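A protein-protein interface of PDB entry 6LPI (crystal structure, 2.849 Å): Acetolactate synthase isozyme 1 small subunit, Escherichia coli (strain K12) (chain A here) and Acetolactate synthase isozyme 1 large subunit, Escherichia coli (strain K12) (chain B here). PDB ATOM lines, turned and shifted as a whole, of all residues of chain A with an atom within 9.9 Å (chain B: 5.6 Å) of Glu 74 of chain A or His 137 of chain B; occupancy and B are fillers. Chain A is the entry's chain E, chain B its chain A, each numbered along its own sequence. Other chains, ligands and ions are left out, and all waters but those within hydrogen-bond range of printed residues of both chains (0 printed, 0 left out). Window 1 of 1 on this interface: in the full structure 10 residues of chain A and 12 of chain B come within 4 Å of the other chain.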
ATOM      1  N   THR A  15      -1.781  31.151 -15.337  1.00  0.00           N
ATOM      2  CA  THR A  15      -1.115  31.986 -16.324  1.00  0.00           C
ATOM      3  C   THR A  15      -0.378  31.090 -17.307  1.00  0.00           C
ATOM      4  O   THR A  15       0.520  30.326 -16.903  1.00  0.00           O
ATOM      5  CB  THR A  15      -0.150  32.965 -15.680  1.00  0.00           C
ATOM      6  OG1 THR A  15      -0.857  33.740 -14.714  1.00  0.00           O
ATOM      7  CG2 THR A  15       0.380  33.886 -16.762  1.00  0.00           C
ATOM      8  N   VAL A  16      -0.758  31.198 -18.589  1.00  0.00           N
ATOM      9  CA  VAL A  16      -0.291  30.307 -19.647  1.00  0.00           C
ATOM     10  C   VAL A  16       0.235  31.128 -20.813  1.00  0.00           C
ATOM     11  O   VAL A  16      -0.114  32.293 -20.990  1.00  0.00           O
ATOM     12  CB  VAL A  16      -1.394  29.357 -20.152  1.00  0.00           C
ATOM     13  CG1 VAL A  16      -1.922  28.495 -19.016  1.00  0.00           C
ATOM     14  CG2 VAL A  16      -2.521  30.138 -20.818  1.00  0.00           C
ATOM     15  N   ARG A  17       1.090  30.500 -21.611  1.00  0.00           N
ATOM     16  CA  ARG A  17       1.587  31.126 -22.828  1.00  0.00           C
ATOM     17  C   ARG A  17       0.483  31.107 -23.874  1.00  0.00           C
ATOM     18  O   ARG A  17      -0.252  30.123 -23.998  1.00  0.00           O
ATOM     19  CB  ARG A  17       2.839  30.402 -23.333  1.00  0.00           C
ATOM     20  CG  ARG A  17       3.813  30.077 -22.210  1.00  0.00           C
ATOM     21  CD  ARG A  17       5.278  30.161 -22.619  1.00  0.00           C
ATOM     22  NE  ARG A  17       5.745  28.929 -23.259  1.00  0.00           N
ATOM     23  CZ  ARG A  17       6.491  28.001 -22.657  1.00  0.00           C
ATOM     24  NH1 ARG A  17       6.887  26.916 -23.324  1.00  0.00           N
ATOM     25  NH2 ARG A  17       6.842  28.159 -21.385  1.00  0.00           N
ATOM     26  N   ASN A  18       0.327  32.216 -24.598  1.00  0.00           N
ATOM     27  CA  ASN A  18      -0.815  32.346 -25.500  1.00  0.00           C
ATOM     28  C   ASN A  18      -0.391  31.865 -26.876  1.00  0.00           C
ATOM     29  O   ASN A  18       0.291  32.576 -27.615  1.00  0.00           O
ATOM     30  CB  ASN A  18      -1.334  33.778 -25.546  1.00  0.00           C
ATOM     31  CG  ASN A  18      -2.601  33.922 -26.405  1.00  0.00           C
ATOM     32  OD1 ASN A  18      -3.138  32.940 -26.924  1.00  0.00           O
ATOM     33  ND2 ASN A  18      -3.077  35.154 -26.549  1.00  0.00           N
ATOM     34  N   HIS A  19      -0.795  30.649 -27.218  1.00  0.00           N
ATOM     35  CA  HIS A  19      -0.642  30.122 -28.563  1.00  0.00           C
ATOM     36  C   HIS A  19      -1.798  29.165 -28.814  1.00  0.00           C
ATOM     37  O   HIS A  19      -2.422  28.682 -27.861  1.00  0.00           O
ATOM     38  CB  HIS A  19       0.707  29.407 -28.736  1.00  0.00           C
ATOM     39  CG  HIS A  19       0.794  28.090 -28.022  1.00  0.00           C
ATOM     40  ND1 HIS A  19       0.355  26.910 -28.581  1.00  0.00           N
ATOM     41  CD2 HIS A  19       1.251  27.773 -26.788  1.00  0.00           C
ATOM     42  CE1 HIS A  19       0.537  25.922 -27.722  1.00  0.00           C
ATOM     43  NE2 HIS A  19       1.088  26.419 -26.630  1.00  0.00           N
ATOM     44  N   PRO A  20      -2.113  28.869 -30.081  1.00  0.00           N
ATOM     45  CA  PRO A  20      -3.207  27.925 -30.356  1.00  0.00           C
ATOM     46  C   PRO A  20      -2.720  26.487 -30.502  1.00  0.00           C
ATOM     47  O   PRO A  20      -2.016  26.157 -31.474  1.00  0.00           O
ATOM     48  CB  PRO A  20      -3.778  28.456 -31.675  1.00  0.00           C
ATOM     49  CG  PRO A  20      -2.561  29.067 -32.389  1.00  0.00           C
ATOM     50  CD  PRO A  20      -1.618  29.535 -31.306  1.00  0.00           C
ATOM     51  N   GLY A  21      -3.085  25.609 -29.571  1.00  0.00           N
ATOM     52  CA  GLY A  21      -3.945  25.932 -28.475  1.00  0.00           C
ATOM     53  C   GLY A  21      -3.427  25.311 -27.195  1.00  0.00           C
ATOM     54  O   GLY A  21      -3.410  24.076 -27.010  1.00  0.00           O
ATOM     55  N   VAL A  22      -2.972  26.198 -26.308  1.00  0.00           N
ATOM     56  CA  VAL A  22      -2.782  25.829 -24.916  1.00  0.00           C
ATOM     57  C   VAL A  22      -4.118  25.399 -24.309  1.00  0.00           C
ATOM     58  O   VAL A  22      -4.158  24.555 -23.398  1.00  0.00           O
ATOM     59  CB  VAL A  22      -2.152  27.012 -24.151  1.00  0.00           C
ATOM     60  CG1 VAL A  22      -3.062  28.216 -24.232  1.00  0.00           C
ATOM     61  CG2 VAL A  22      -1.844  26.664 -22.699  1.00  0.00           C
ATOM     62  N   HIS A  25      -4.615  21.804 -24.625  1.00  0.00           N
ATOM     63  CA  HIS A  25      -3.805  21.155 -23.602  1.00  0.00           C
ATOM     64  C   HIS A  25      -4.535  21.102 -22.271  1.00  0.00           C
ATOM     65  O   HIS A  25      -4.661  20.040 -21.660  1.00  0.00           O
ATOM     66  CB  HIS A  25      -2.495  21.908 -23.432  1.00  0.00           C
ATOM     67  CG  HIS A  25      -1.363  21.329 -24.210  1.00  0.00           C
ATOM     68  ND1 HIS A  25      -0.726  20.166 -23.835  1.00  0.00           N
ATOM     69  CD2 HIS A  25      -0.737  21.757 -25.332  1.00  0.00           C
ATOM     70  CE1 HIS A  25       0.253  19.908 -24.686  1.00  0.00           C
ATOM     71  NE2 HIS A  25       0.269  20.857 -25.605  1.00  0.00           N
ATOM     72  N   VAL A  26      -5.011  22.251 -21.796  1.00  0.00           N
ATOM     73  CA  VAL A  26      -5.547  22.333 -20.440  1.00  0.00           C
ATOM     74  C   VAL A  26      -6.895  21.630 -20.350  1.00  0.00           C
ATOM     75  O   VAL A  26      -7.123  20.785 -19.465  1.00  0.00           O
ATOM     76  CB  VAL A  26      -5.636  23.807 -20.002  1.00  0.00           C
ATOM     77  CG1 VAL A  26      -6.471  23.946 -18.747  1.00  0.00           C
ATOM     78  CG2 VAL A  26      -4.228  24.397 -19.832  1.00  0.00           C
ATOM     79  N   LEU A  29      -6.360  17.944 -20.518  1.00  0.00           N
ATOM     80  CA  LEU A  29      -5.905  17.444 -19.225  1.00  0.00           C
ATOM     81  C   LEU A  29      -7.069  17.242 -18.274  1.00  0.00           C
ATOM     82  O   LEU A  29      -7.145  16.213 -17.593  1.00  0.00           O
ATOM     83  CB  LEU A  29      -4.883  18.398 -18.604  1.00  0.00           C
ATOM     84  CG  LEU A  29      -4.532  18.081 -17.155  1.00  0.00           C
ATOM     85  CD1 LEU A  29      -3.543  16.994 -17.054  1.00  0.00           C
ATOM     86  CD2 LEU A  29      -3.985  19.315 -16.473  1.00  0.00           C
ATOM     87  N   ARG A  32      -9.143  14.200 -19.541  1.00  0.00           N
ATOM     88  CA  ARG A  32      -8.388  12.953 -19.507  1.00  0.00           C
ATOM     89  C   ARG A  32      -8.297  12.392 -18.101  1.00  0.00           C
ATOM     90  O   ARG A  32      -8.393  11.178 -17.916  1.00  0.00           O
ATOM     91  CB  ARG A  32      -7.010  13.226 -20.119  1.00  0.00           C
ATOM     92  CG  ARG A  32      -5.835  12.387 -19.760  1.00  0.00           C
ATOM     93  CD  ARG A  32      -4.553  13.084 -20.345  1.00  0.00           C
ATOM     94  NE  ARG A  32      -4.831  13.744 -21.620  1.00  0.00           N
ATOM     95  CZ  ARG A  32      -4.335  14.918 -21.991  1.00  0.00           C
ATOM     96  NH1 ARG A  32      -3.536  15.601 -21.167  1.00  0.00           N
ATOM     97  NH2 ARG A  32      -4.680  15.425 -23.176  1.00  0.00           N
ATOM     98  N   LYS A  50       0.802  36.300 -22.880  1.00  0.00           N
ATOM     99  CA  LYS A  50       0.208  35.305 -22.005  1.00  0.00           C
ATOM    100  C   LYS A  50      -1.294  35.503 -21.919  1.00  0.00           C
ATOM    101  O   LYS A  50      -1.830  36.561 -22.257  1.00  0.00           O
ATOM    102  CB  LYS A  50       0.809  35.352 -20.598  1.00  0.00           C
ATOM    103  CG  LYS A  50       2.216  35.860 -20.556  1.00  0.00           C
ATOM    104  CD  LYS A  50       3.209  34.737 -20.721  1.00  0.00           C
ATOM    105  CE  LYS A  50       4.528  35.094 -20.043  1.00  0.00           C
ATOM    106  NZ  LYS A  50       5.703  34.532 -20.783  1.00  0.00           N
ATOM    107  N   SER A  68      -0.583  19.816  -9.144  1.00  0.00           N
ATOM    108  CA  SER A  68       0.625  19.147  -9.616  1.00  0.00           C
ATOM    109  C   SER A  68       0.494  18.738 -11.096  1.00  0.00           C
ATOM    110  O   SER A  68       1.385  19.018 -11.930  1.00  0.00           O
ATOM    111  CB  SER A  68       0.910  17.940  -8.721  1.00  0.00           C
ATOM    112  OG  SER A  68       1.298  18.305  -7.399  1.00  0.00           O
ATOM    113  N   GLN A  69      -0.624  18.086 -11.443  1.00  0.00           N
ATOM    114  CA  GLN A  69      -0.860  17.725 -12.835  1.00  0.00           C
ATOM    115  C   GLN A  69      -0.765  18.946 -13.734  1.00  0.00           C
ATOM    116  O   GLN A  69      -0.008  18.943 -14.711  1.00  0.00           O
ATOM    117  CB  GLN A  69      -2.224  17.044 -13.000  1.00  0.00           C
ATOM    118  CG  GLN A  69      -2.315  15.684 -12.353  1.00  0.00           C
ATOM    119  CD  GLN A  69      -1.236  14.715 -12.818  1.00  0.00           C
ATOM    120  OE1 GLN A  69      -0.801  13.850 -12.057  1.00  0.00           O
ATOM    121  NE2 GLN A  69      -0.817  14.840 -14.075  1.00  0.00           N
ATOM    122  N   ILE A  70      -1.505  20.015 -13.401  1.00  0.00           N
ATOM    123  CA  ILE A  70      -1.529  21.198 -14.265  1.00  0.00           C
ATOM    124  C   ILE A  70      -0.136  21.793 -14.411  1.00  0.00           C
ATOM    125  O   ILE A  70       0.253  22.240 -15.501  1.00  0.00           O
ATOM    126  CB  ILE A  70      -2.527  22.242 -13.741  1.00  0.00           C
ATOM    127  CG1 ILE A  70      -3.932  21.655 -13.758  1.00  0.00           C
ATOM    128  CG2 ILE A  70      -2.511  23.467 -14.629  1.00  0.00           C
ATOM    129  CD1 ILE A  70      -4.934  22.444 -12.982  1.00  0.00           C
ATOM    130  N   ASP A  71       0.644  21.796 -13.326  1.00  0.00           N
ATOM    131  CA  ASP A  71       1.983  22.363 -13.407  1.00  0.00           C
ATOM    132  C   ASP A  71       2.938  21.514 -14.244  1.00  0.00           C
ATOM    133  O   ASP A  71       3.993  22.017 -14.659  1.00  0.00           O
ATOM    134  CB  ASP A  71       2.559  22.592 -12.022  1.00  0.00           C
ATOM    135  CG  ASP A  71       3.459  23.795 -11.988  1.00  0.00           C
ATOM    136  OD1 ASP A  71       3.945  24.211 -13.071  1.00  0.00           O
ATOM    137  OD2 ASP A  71       3.684  24.332 -10.896  1.00  0.00           O
ATOM    138  N   LYS A  72       2.585  20.257 -14.526  1.00  0.00           N
ATOM    139  CA  LYS A  72       3.347  19.489 -15.509  1.00  0.00           C
ATOM    140  C   LYS A  72       3.275  20.066 -16.935  1.00  0.00           C
ATOM    141  O   LYS A  72       4.166  19.783 -17.748  1.00  0.00           O
ATOM    142  CB  LYS A  72       2.866  18.038 -15.499  1.00  0.00           C
ATOM    143  CG  LYS A  72       3.293  17.258 -14.254  1.00  0.00           C
ATOM    144  CD  LYS A  72       2.503  15.943 -14.098  1.00  0.00           C
ATOM    145  CE  LYS A  72       2.768  14.976 -15.269  1.00  0.00           C
ATOM    146  NZ  LYS A  72       4.086  14.337 -15.116  1.00  0.00           N
ATOM    147  N   LEU A  73       2.257  20.858 -17.277  1.00  0.00           N
ATOM    148  CA  LEU A  73       2.164  21.374 -18.644  1.00  0.00           C
ATOM    149  C   LEU A  73       3.220  22.452 -18.898  1.00  0.00           C
ATOM    150  O   LEU A  73       3.371  23.384 -18.106  1.00  0.00           O
ATOM    151  CB  LEU A  73       0.770  21.936 -18.906  1.00  0.00           C
ATOM    152  CG  LEU A  73      -0.424  21.033 -18.596  1.00  0.00           C
ATOM    153  CD1 LEU A  73      -1.705  21.792 -18.832  1.00  0.00           C
ATOM    154  CD2 LEU A  73      -0.371  19.835 -19.446  1.00  0.00           C
ATOM    155  N   GLU A  74       3.957  22.335 -20.010  1.00  0.00           N
ATOM    156  CA  GLU A  74       5.030  23.297 -20.257  1.00  0.00           C
ATOM    157  C   GLU A  74       4.483  24.711 -20.363  1.00  0.00           C
ATOM    158  O   GLU A  74       5.048  25.646 -19.782  1.00  0.00           O
ATOM    159  CB  GLU A  74       5.816  22.946 -21.524  1.00  0.00           C
ATOM    160  CG  GLU A  74       6.968  21.950 -21.284  1.00  0.00           C
ATOM    161  CD  GLU A  74       8.197  22.559 -20.573  1.00  0.00           C
ATOM    162  OE1 GLU A  74       8.809  23.518 -21.109  1.00  0.00           O
ATOM    163  OE2 GLU A  74       8.557  22.061 -19.479  1.00  0.00           O
ATOM    164  N   ASP A  75       3.363  24.882 -21.070  1.00  0.00           N
ATOM    165  CA  ASP A  75       2.853  26.216 -21.345  1.00  0.00           C
ATOM    166  C   ASP A  75       2.288  26.914 -20.125  1.00  0.00           C
ATOM    167  O   ASP A  75       2.059  28.122 -20.190  1.00  0.00           O
ATOM    168  CB  ASP A  75       1.798  26.155 -22.452  1.00  0.00           C
ATOM    169  CG  ASP A  75       2.407  25.867 -23.813  1.00  0.00           C
ATOM    170  OD1 ASP A  75       1.794  25.096 -24.576  1.00  0.00           O
ATOM    171  OD2 ASP A  75       3.519  26.388 -24.109  1.00  0.00           O
ATOM    172  N   VAL A  76       2.063  26.204 -19.024  1.00  0.00           N
ATOM    173  CA  VAL A  76       1.541  26.816 -17.804  1.00  0.00           C
ATOM    174  C   VAL A  76       2.710  27.490 -17.094  1.00  0.00           C
ATOM    175  O   VAL A  76       3.664  26.832 -16.673  1.00  0.00           O
ATOM    176  CB  VAL A  76       0.847  25.789 -16.902  1.00  0.00           C
ATOM    177  CG1 VAL A  76       0.887  26.219 -15.465  1.00  0.00           C
ATOM    178  CG2 VAL A  76      -0.594  25.621 -17.328  1.00  0.00           C
ATOM    179  N   VAL A  77       2.654  28.812 -16.998  1.00  0.00           N
ATOM    180  CA  VAL A  77       3.709  29.562 -16.341  1.00  0.00           C
ATOM    181  C   VAL A  77       3.450  29.668 -14.845  1.00  0.00           C
ATOM    182  O   VAL A  77       4.403  29.794 -14.063  1.00  0.00           O
ATOM    183  CB  VAL A  77       3.836  30.939 -17.003  1.00  0.00           C
ATOM    184  CG1 VAL A  77       4.579  31.918 -16.122  1.00  0.00           C
ATOM    185  CG2 VAL A  77       4.527  30.791 -18.338  1.00  0.00           C
ATOM    186  N   LYS A  78       2.177  29.606 -14.432  1.00  0.00           N
ATOM    187  CA  LYS A  78       1.847  29.677 -13.011  1.00  0.00           C
ATOM    188  C   LYS A  78       0.431  29.163 -12.813  1.00  0.00           C
ATOM    189  O   LYS A  78      -0.386  29.190 -13.736  1.00  0.00           O
ATOM    190  CB  LYS A  78       2.010  31.105 -12.485  1.00  0.00           C
ATOM    191  CG  LYS A  78       1.388  31.419 -11.137  1.00  0.00           C
ATOM    192  CD  LYS A  78       0.318  32.502 -11.292  1.00  0.00           C
ATOM    193  CE  LYS A  78      -0.907  31.949 -12.038  1.00  0.00           C
ATOM    194  NZ  LYS A  78      -1.960  32.930 -12.395  1.00  0.00           N
ATOM    195  N   TYR B 128      -0.618  17.729 -34.197  1.00  0.00           N
ATOM    196  CA  TYR B 128      -0.530  18.381 -32.895  1.00  0.00           C
ATOM    197  C   TYR B 128      -1.607  17.856 -31.958  1.00  0.00           C
ATOM    198  O   TYR B 128      -1.337  17.463 -30.810  1.00  0.00           O
ATOM    199  CB  TYR B 128      -0.734  19.886 -33.041  1.00  0.00           C
ATOM    200  CG  TYR B 128      -0.350  20.675 -31.806  1.00  0.00           C
ATOM    201  CD1 TYR B 128      -1.327  21.035 -30.879  1.00  0.00           C
ATOM    202  CD2 TYR B 128       0.979  21.033 -31.542  1.00  0.00           C
ATOM    203  CE1 TYR B 128      -1.002  21.755 -29.732  1.00  0.00           C
ATOM    204  CE2 TYR B 128       1.314  21.756 -30.405  1.00  0.00           C
ATOM    205  CZ  TYR B 128       0.301  22.115 -29.494  1.00  0.00           C
ATOM    206  OH  TYR B 128       0.581  22.836 -28.348  1.00  0.00           O
ATOM    207  N   THR B 135       2.256  12.964 -25.161  1.00  0.00           N
ATOM    208  CA  THR B 135       3.605  13.495 -25.174  1.00  0.00           C
ATOM    209  C   THR B 135       3.886  14.199 -23.859  1.00  0.00           C
ATOM    210  O   THR B 135       2.973  14.649 -23.182  1.00  0.00           O
ATOM    211  CB  THR B 135       3.790  14.455 -26.318  1.00  0.00           C
ATOM    212  OG1 THR B 135       2.643  15.313 -26.367  1.00  0.00           O
ATOM    213  CG2 THR B 135       3.839  13.654 -27.589  1.00  0.00           C
ATOM    214  N   LYS B 136       5.164  14.288 -23.490  1.00  0.00           N
ATOM    215  CA  LYS B 136       5.518  15.201 -22.410  1.00  0.00           C
ATOM    216  C   LYS B 136       5.386  16.659 -22.848  1.00  0.00           C
ATOM    217  O   LYS B 136       5.110  17.526 -22.015  1.00  0.00           O
ATOM    218  CB  LYS B 136       6.941  14.920 -21.903  1.00  0.00           C
ATOM    219  CG  LYS B 136       7.295  15.799 -20.727  1.00  0.00           C
ATOM    220  CD  LYS B 136       8.763  15.888 -20.471  1.00  0.00           C
ATOM    221  CE  LYS B 136       9.034  15.954 -19.009  1.00  0.00           C
ATOM    222  NZ  LYS B 136      10.441  16.221 -18.669  1.00  0.00           N
ATOM    223  N   HIS B 137       5.605  16.954 -24.127  1.00  0.00           N
ATOM    224  CA  HIS B 137       5.211  18.234 -24.720  1.00  0.00           C
ATOM    225  C   HIS B 137       5.307  18.106 -26.241  1.00  0.00           C
ATOM    226  O   HIS B 137       5.928  17.169 -26.748  1.00  0.00           O
ATOM    227  CB  HIS B 137       6.091  19.382 -24.213  1.00  0.00           C
ATOM    228  CG  HIS B 137       5.574  20.734 -24.565  1.00  0.00           C
ATOM    229  ND1 HIS B 137       4.228  21.036 -24.587  1.00  0.00           N
ATOM    230  CD2 HIS B 137       6.223  21.872 -24.903  1.00  0.00           C
ATOM    231  CE1 HIS B 137       4.070  22.310 -24.911  1.00  0.00           C
ATOM    232  NE2 HIS B 137       5.266  22.841 -25.105  1.00  0.00           N
ATOM    233  N   ASN B 138       4.696  19.039 -26.972  1.00  0.00           N
ATOM    234  CA  ASN B 138       4.722  18.924 -28.427  1.00  0.00           C
ATOM    235  C   ASN B 138       4.724  20.310 -29.056  1.00  0.00           C
ATOM    236  O   ASN B 138       4.505  21.312 -28.378  1.00  0.00           O
ATOM    237  CB  ASN B 138       3.554  18.083 -28.944  1.00  0.00           C
ATOM    238  CG  ASN B 138       2.220  18.765 -28.750  1.00  0.00           C
ATOM    239  OD1 ASN B 138       2.100  19.695 -27.955  1.00  0.00           O
ATOM    240  ND2 ASN B 138       1.209  18.321 -29.488  1.00  0.00           N
ATOM    241  N   TYR B 139       5.013  20.373 -30.361  1.00  0.00           N
ATOM    242  CA  TYR B 139       5.143  21.669 -31.030  1.00  0.00           C
ATOM    243  C   TYR B 139       4.590  21.614 -32.444  1.00  0.00           C
ATOM    244  O   TYR B 139       4.693  20.593 -33.129  1.00  0.00           O
ATOM    245  CB  TYR B 139       6.584  22.154 -31.137  1.00  0.00           C
ATOM    246  CG  TYR B 139       7.268  22.400 -29.827  1.00  0.00           C
ATOM    247  CD1 TYR B 139       8.086  21.406 -29.266  1.00  0.00           C
ATOM    248  CD2 TYR B 139       7.127  23.605 -29.152  1.00  0.00           C
ATOM    249  CE1 TYR B 139       8.735  21.599 -28.060  1.00  0.00           C
ATOM    250  CE2 TYR B 139       7.785  23.816 -27.938  1.00  0.00           C
ATOM    251  CZ  TYR B 139       8.583  22.805 -27.395  1.00  0.00           C
ATOM    252  OH  TYR B 139       9.238  22.978 -26.195  1.00  0.00           O
ATOM    253  N   ARG B 156      15.662  19.803 -24.088  1.00  0.00           N
ATOM    254  CA  ARG B 156      15.680  19.978 -22.642  1.00  0.00           C
ATOM    255  C   ARG B 156      14.512  19.211 -22.029  1.00  0.00           C
ATOM    256  O   ARG B 156      14.699  18.354 -21.152  1.00  0.00           O
ATOM    257  CB  ARG B 156      15.639  21.470 -22.287  1.00  0.00           C
ATOM    258  CG  ARG B 156      15.649  21.794 -20.791  1.00  0.00           C
ATOM    259  CD  ARG B 156      15.426  23.287 -20.496  1.00  0.00           C
ATOM    260  NE  ARG B 156      14.145  23.781 -21.024  1.00  0.00           N
ATOM    261  CZ  ARG B 156      12.976  23.753 -20.372  1.00  0.00           C
ATOM    262  NH1 ARG B 156      12.886  23.237 -19.145  1.00  0.00           N
ATOM    263  NH2 ARG B 156      11.878  24.231 -20.958  1.00  0.00           N
ATOM    264  N   ILE B 157      13.312  19.420 -22.575  1.00  0.00           N
ATOM    265  CA  ILE B 157      12.109  18.846 -21.982  1.00  0.00           C
ATOM    266  C   ILE B 157      12.167  17.326 -22.004  1.00  0.00           C
ATOM    267  O   ILE B 157      11.824  16.663 -21.024  1.00  0.00           O
ATOM    268  CB  ILE B 157      10.873  19.355 -22.738  1.00  0.00           C
ATOM    269  CG1 ILE B 157      10.718  20.863 -22.595  1.00  0.00           C
ATOM    270  CG2 ILE B 157       9.652  18.573 -22.344  1.00  0.00           C
ATOM    271  CD1 ILE B 157       9.742  21.453 -23.588  1.00  0.00           C
ATOM    272  N   PRO B 165       8.740  11.700 -24.250  1.00  0.00           N
ATOM    273  CA  PRO B 165       8.803  12.077 -25.662  1.00  0.00           C
ATOM    274  C   PRO B 165       8.285  13.481 -25.900  1.00  0.00           C
ATOM    275  O   PRO B 165       7.326  13.938 -25.272  1.00  0.00           O
ATOM    276  CB  PRO B 165       7.885  11.054 -26.338  1.00  0.00           C
ATOM    277  CG  PRO B 165       6.875  10.721 -25.279  1.00  0.00           C
ATOM    278  CD  PRO B 165       7.638  10.765 -23.973  1.00  0.00           C
ATOM    279  N   VAL B 166       8.948  14.173 -26.810  1.00  0.00           N
ATOM    280  CA  VAL B 166       8.483  15.447 -27.320  1.00  0.00           C
ATOM    281  C   VAL B 166       8.337  15.305 -28.824  1.00  0.00           C
ATOM    282  O   VAL B 166       9.211  14.745 -29.504  1.00  0.00           O
ATOM    283  CB  VAL B 166       9.430  16.608 -26.973  1.00  0.00           C
ATOM    284  CG1 VAL B 166       8.786  17.928 -27.374  1.00  0.00           C
ATOM    285  CG2 VAL B 166       9.750  16.599 -25.503  1.00  0.00           C
ATOM    286  N   TRP B 167       7.236  15.831 -29.338  1.00  0.00           N
ATOM    287  CA  TRP B 167       6.885  15.705 -30.738  1.00  0.00           C
ATOM    288  C   TRP B 167       7.011  17.084 -31.371  1.00  0.00           C
ATOM    289  O   TRP B 167       6.383  18.046 -30.908  1.00  0.00           O
ATOM    290  CB  TRP B 167       5.469  15.151 -30.870  1.00  0.00           C
ATOM    291  CG  TRP B 167       5.118  14.710 -32.240  1.00  0.00           C
ATOM    292  CD1 TRP B 167       5.463  15.318 -33.411  1.00  0.00           C
ATOM    293  CD2 TRP B 167       4.335  13.570 -32.592  1.00  0.00           C
ATOM    294  NE1 TRP B 167       4.949  14.619 -34.472  1.00  0.00           N
ATOM    295  CE2 TRP B 167       4.255  13.539 -33.997  1.00  0.00           C
ATOM    296  CE3 TRP B 167       3.686  12.570 -31.854  1.00  0.00           C
ATOM    297  CZ2 TRP B 167       3.566  12.550 -34.682  1.00  0.00           C
ATOM    298  CZ3 TRP B 167       2.997  11.579 -32.542  1.00  0.00           C
ATOM    299  CH2 TRP B 167       2.944  11.582 -33.945  1.00  0.00           C
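NE of Arg 17 of chain A lies within salt-bridge range of OD2 of Asp 75 of chain A, at 3.5 Å. The backbone carbonyl oxygen (O) of His 137 of chain B sits at hydrogen-bond distance from the backbone NH (N) of Trp 167 of chain B (3.2 Å). NE2 of His 19 of chain A lies within hydrogen-bond range of OD1 of Asp 75 of chain A. The backbone carbonyl oxygen (O) of Tyr 128 of chain B sits at hydrogen-bond distance from the side-chain amide nitrogen (ND2) of Asn 138 of chain B. The guanidinium group of Arg 17 of chain A lies within hydrogen-bond range of the backbone carbonyl oxygen of Glu 74 of chain A. NZ of Lys 136 of chain B sits at hydrogen-bond distance from O of Ile 157 of chain B (2.8 Å).
The side-chain hydroxyl (OH) of Tyr 128 of chain B sits at hydrogen-bond distance from a ring nitrogen (NE2) of His 25 of chain A. The guanidinium group (NH2) of Arg 156 of chain B is in salt-bridge range of the side-chain carboxylate (OE1) of Glu 74 of chain A. The side-chain amide oxygen of Asn 138 of chain B is in hydrogen-bond range of a ring nitrogen (NE2) of His 25 of chain A, 3.2 Å away.
His 19 of chain A touches Tyr 128 of chain B (CE1 to OH, 3.1 Å). Glu 74 of chain A touches His 137 of chain B (CB to CD2, 3.6 Å). Glu 74 of chain A touches Ile 157 of chain B (OE1 to CD1, 3.4 Å). Asp 75 of chain A touches His 137 of chain B.
Hydrophobic or aromatic side chains of chain B within 4 Å of the printed part of chain A: Tyr 128, His 137 and Ile 157. Of the 24 printed residues of chain A, 4 touch a printed residue of chain B. Printed residues of chain A that touch a printed residue of chain B: His 19, His 25, Glu 74 and Asp 75. Among the printed residues, Asp or Glu carboxylates within 4 Å of a Lys or Arg side-chain nitrogen of the other chain: Glu 74 of chain A with Arg 156 of chain B (3.2 Å).
Of the printed residues of chain B, His 25 of chain A touches Tyr 128 (3.4 Å) and Asn 138 (3.2 Å). Glu 74 of chain A touches just these residues of chain B: His 137, Arg 156 and Ile 157. Of the printed residues of chain B, Asp 75 of chain A touches His 137. Of the printed residues of chain A, Tyr 128 of chain B touches His 19 and His 25. No residue of chain A comes within 4 Å of Thr 135 of chain B. Of the printed residues of chain A, His 137 of chain B touches Glu 74 and Asp 75. Asn 138 of chain B touches just one residue of chain A: His 25. No residue of chain A comes within 4 Å of Val 166 of chain B. The nearest residue of chain A that does not touch His 137 of chain B is His 25 of chain A (4.1 Å). The nearest printed residue of chain B that does not touch Asp 75 of chain A is Tyr 128 of chain B (4.6 Å).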
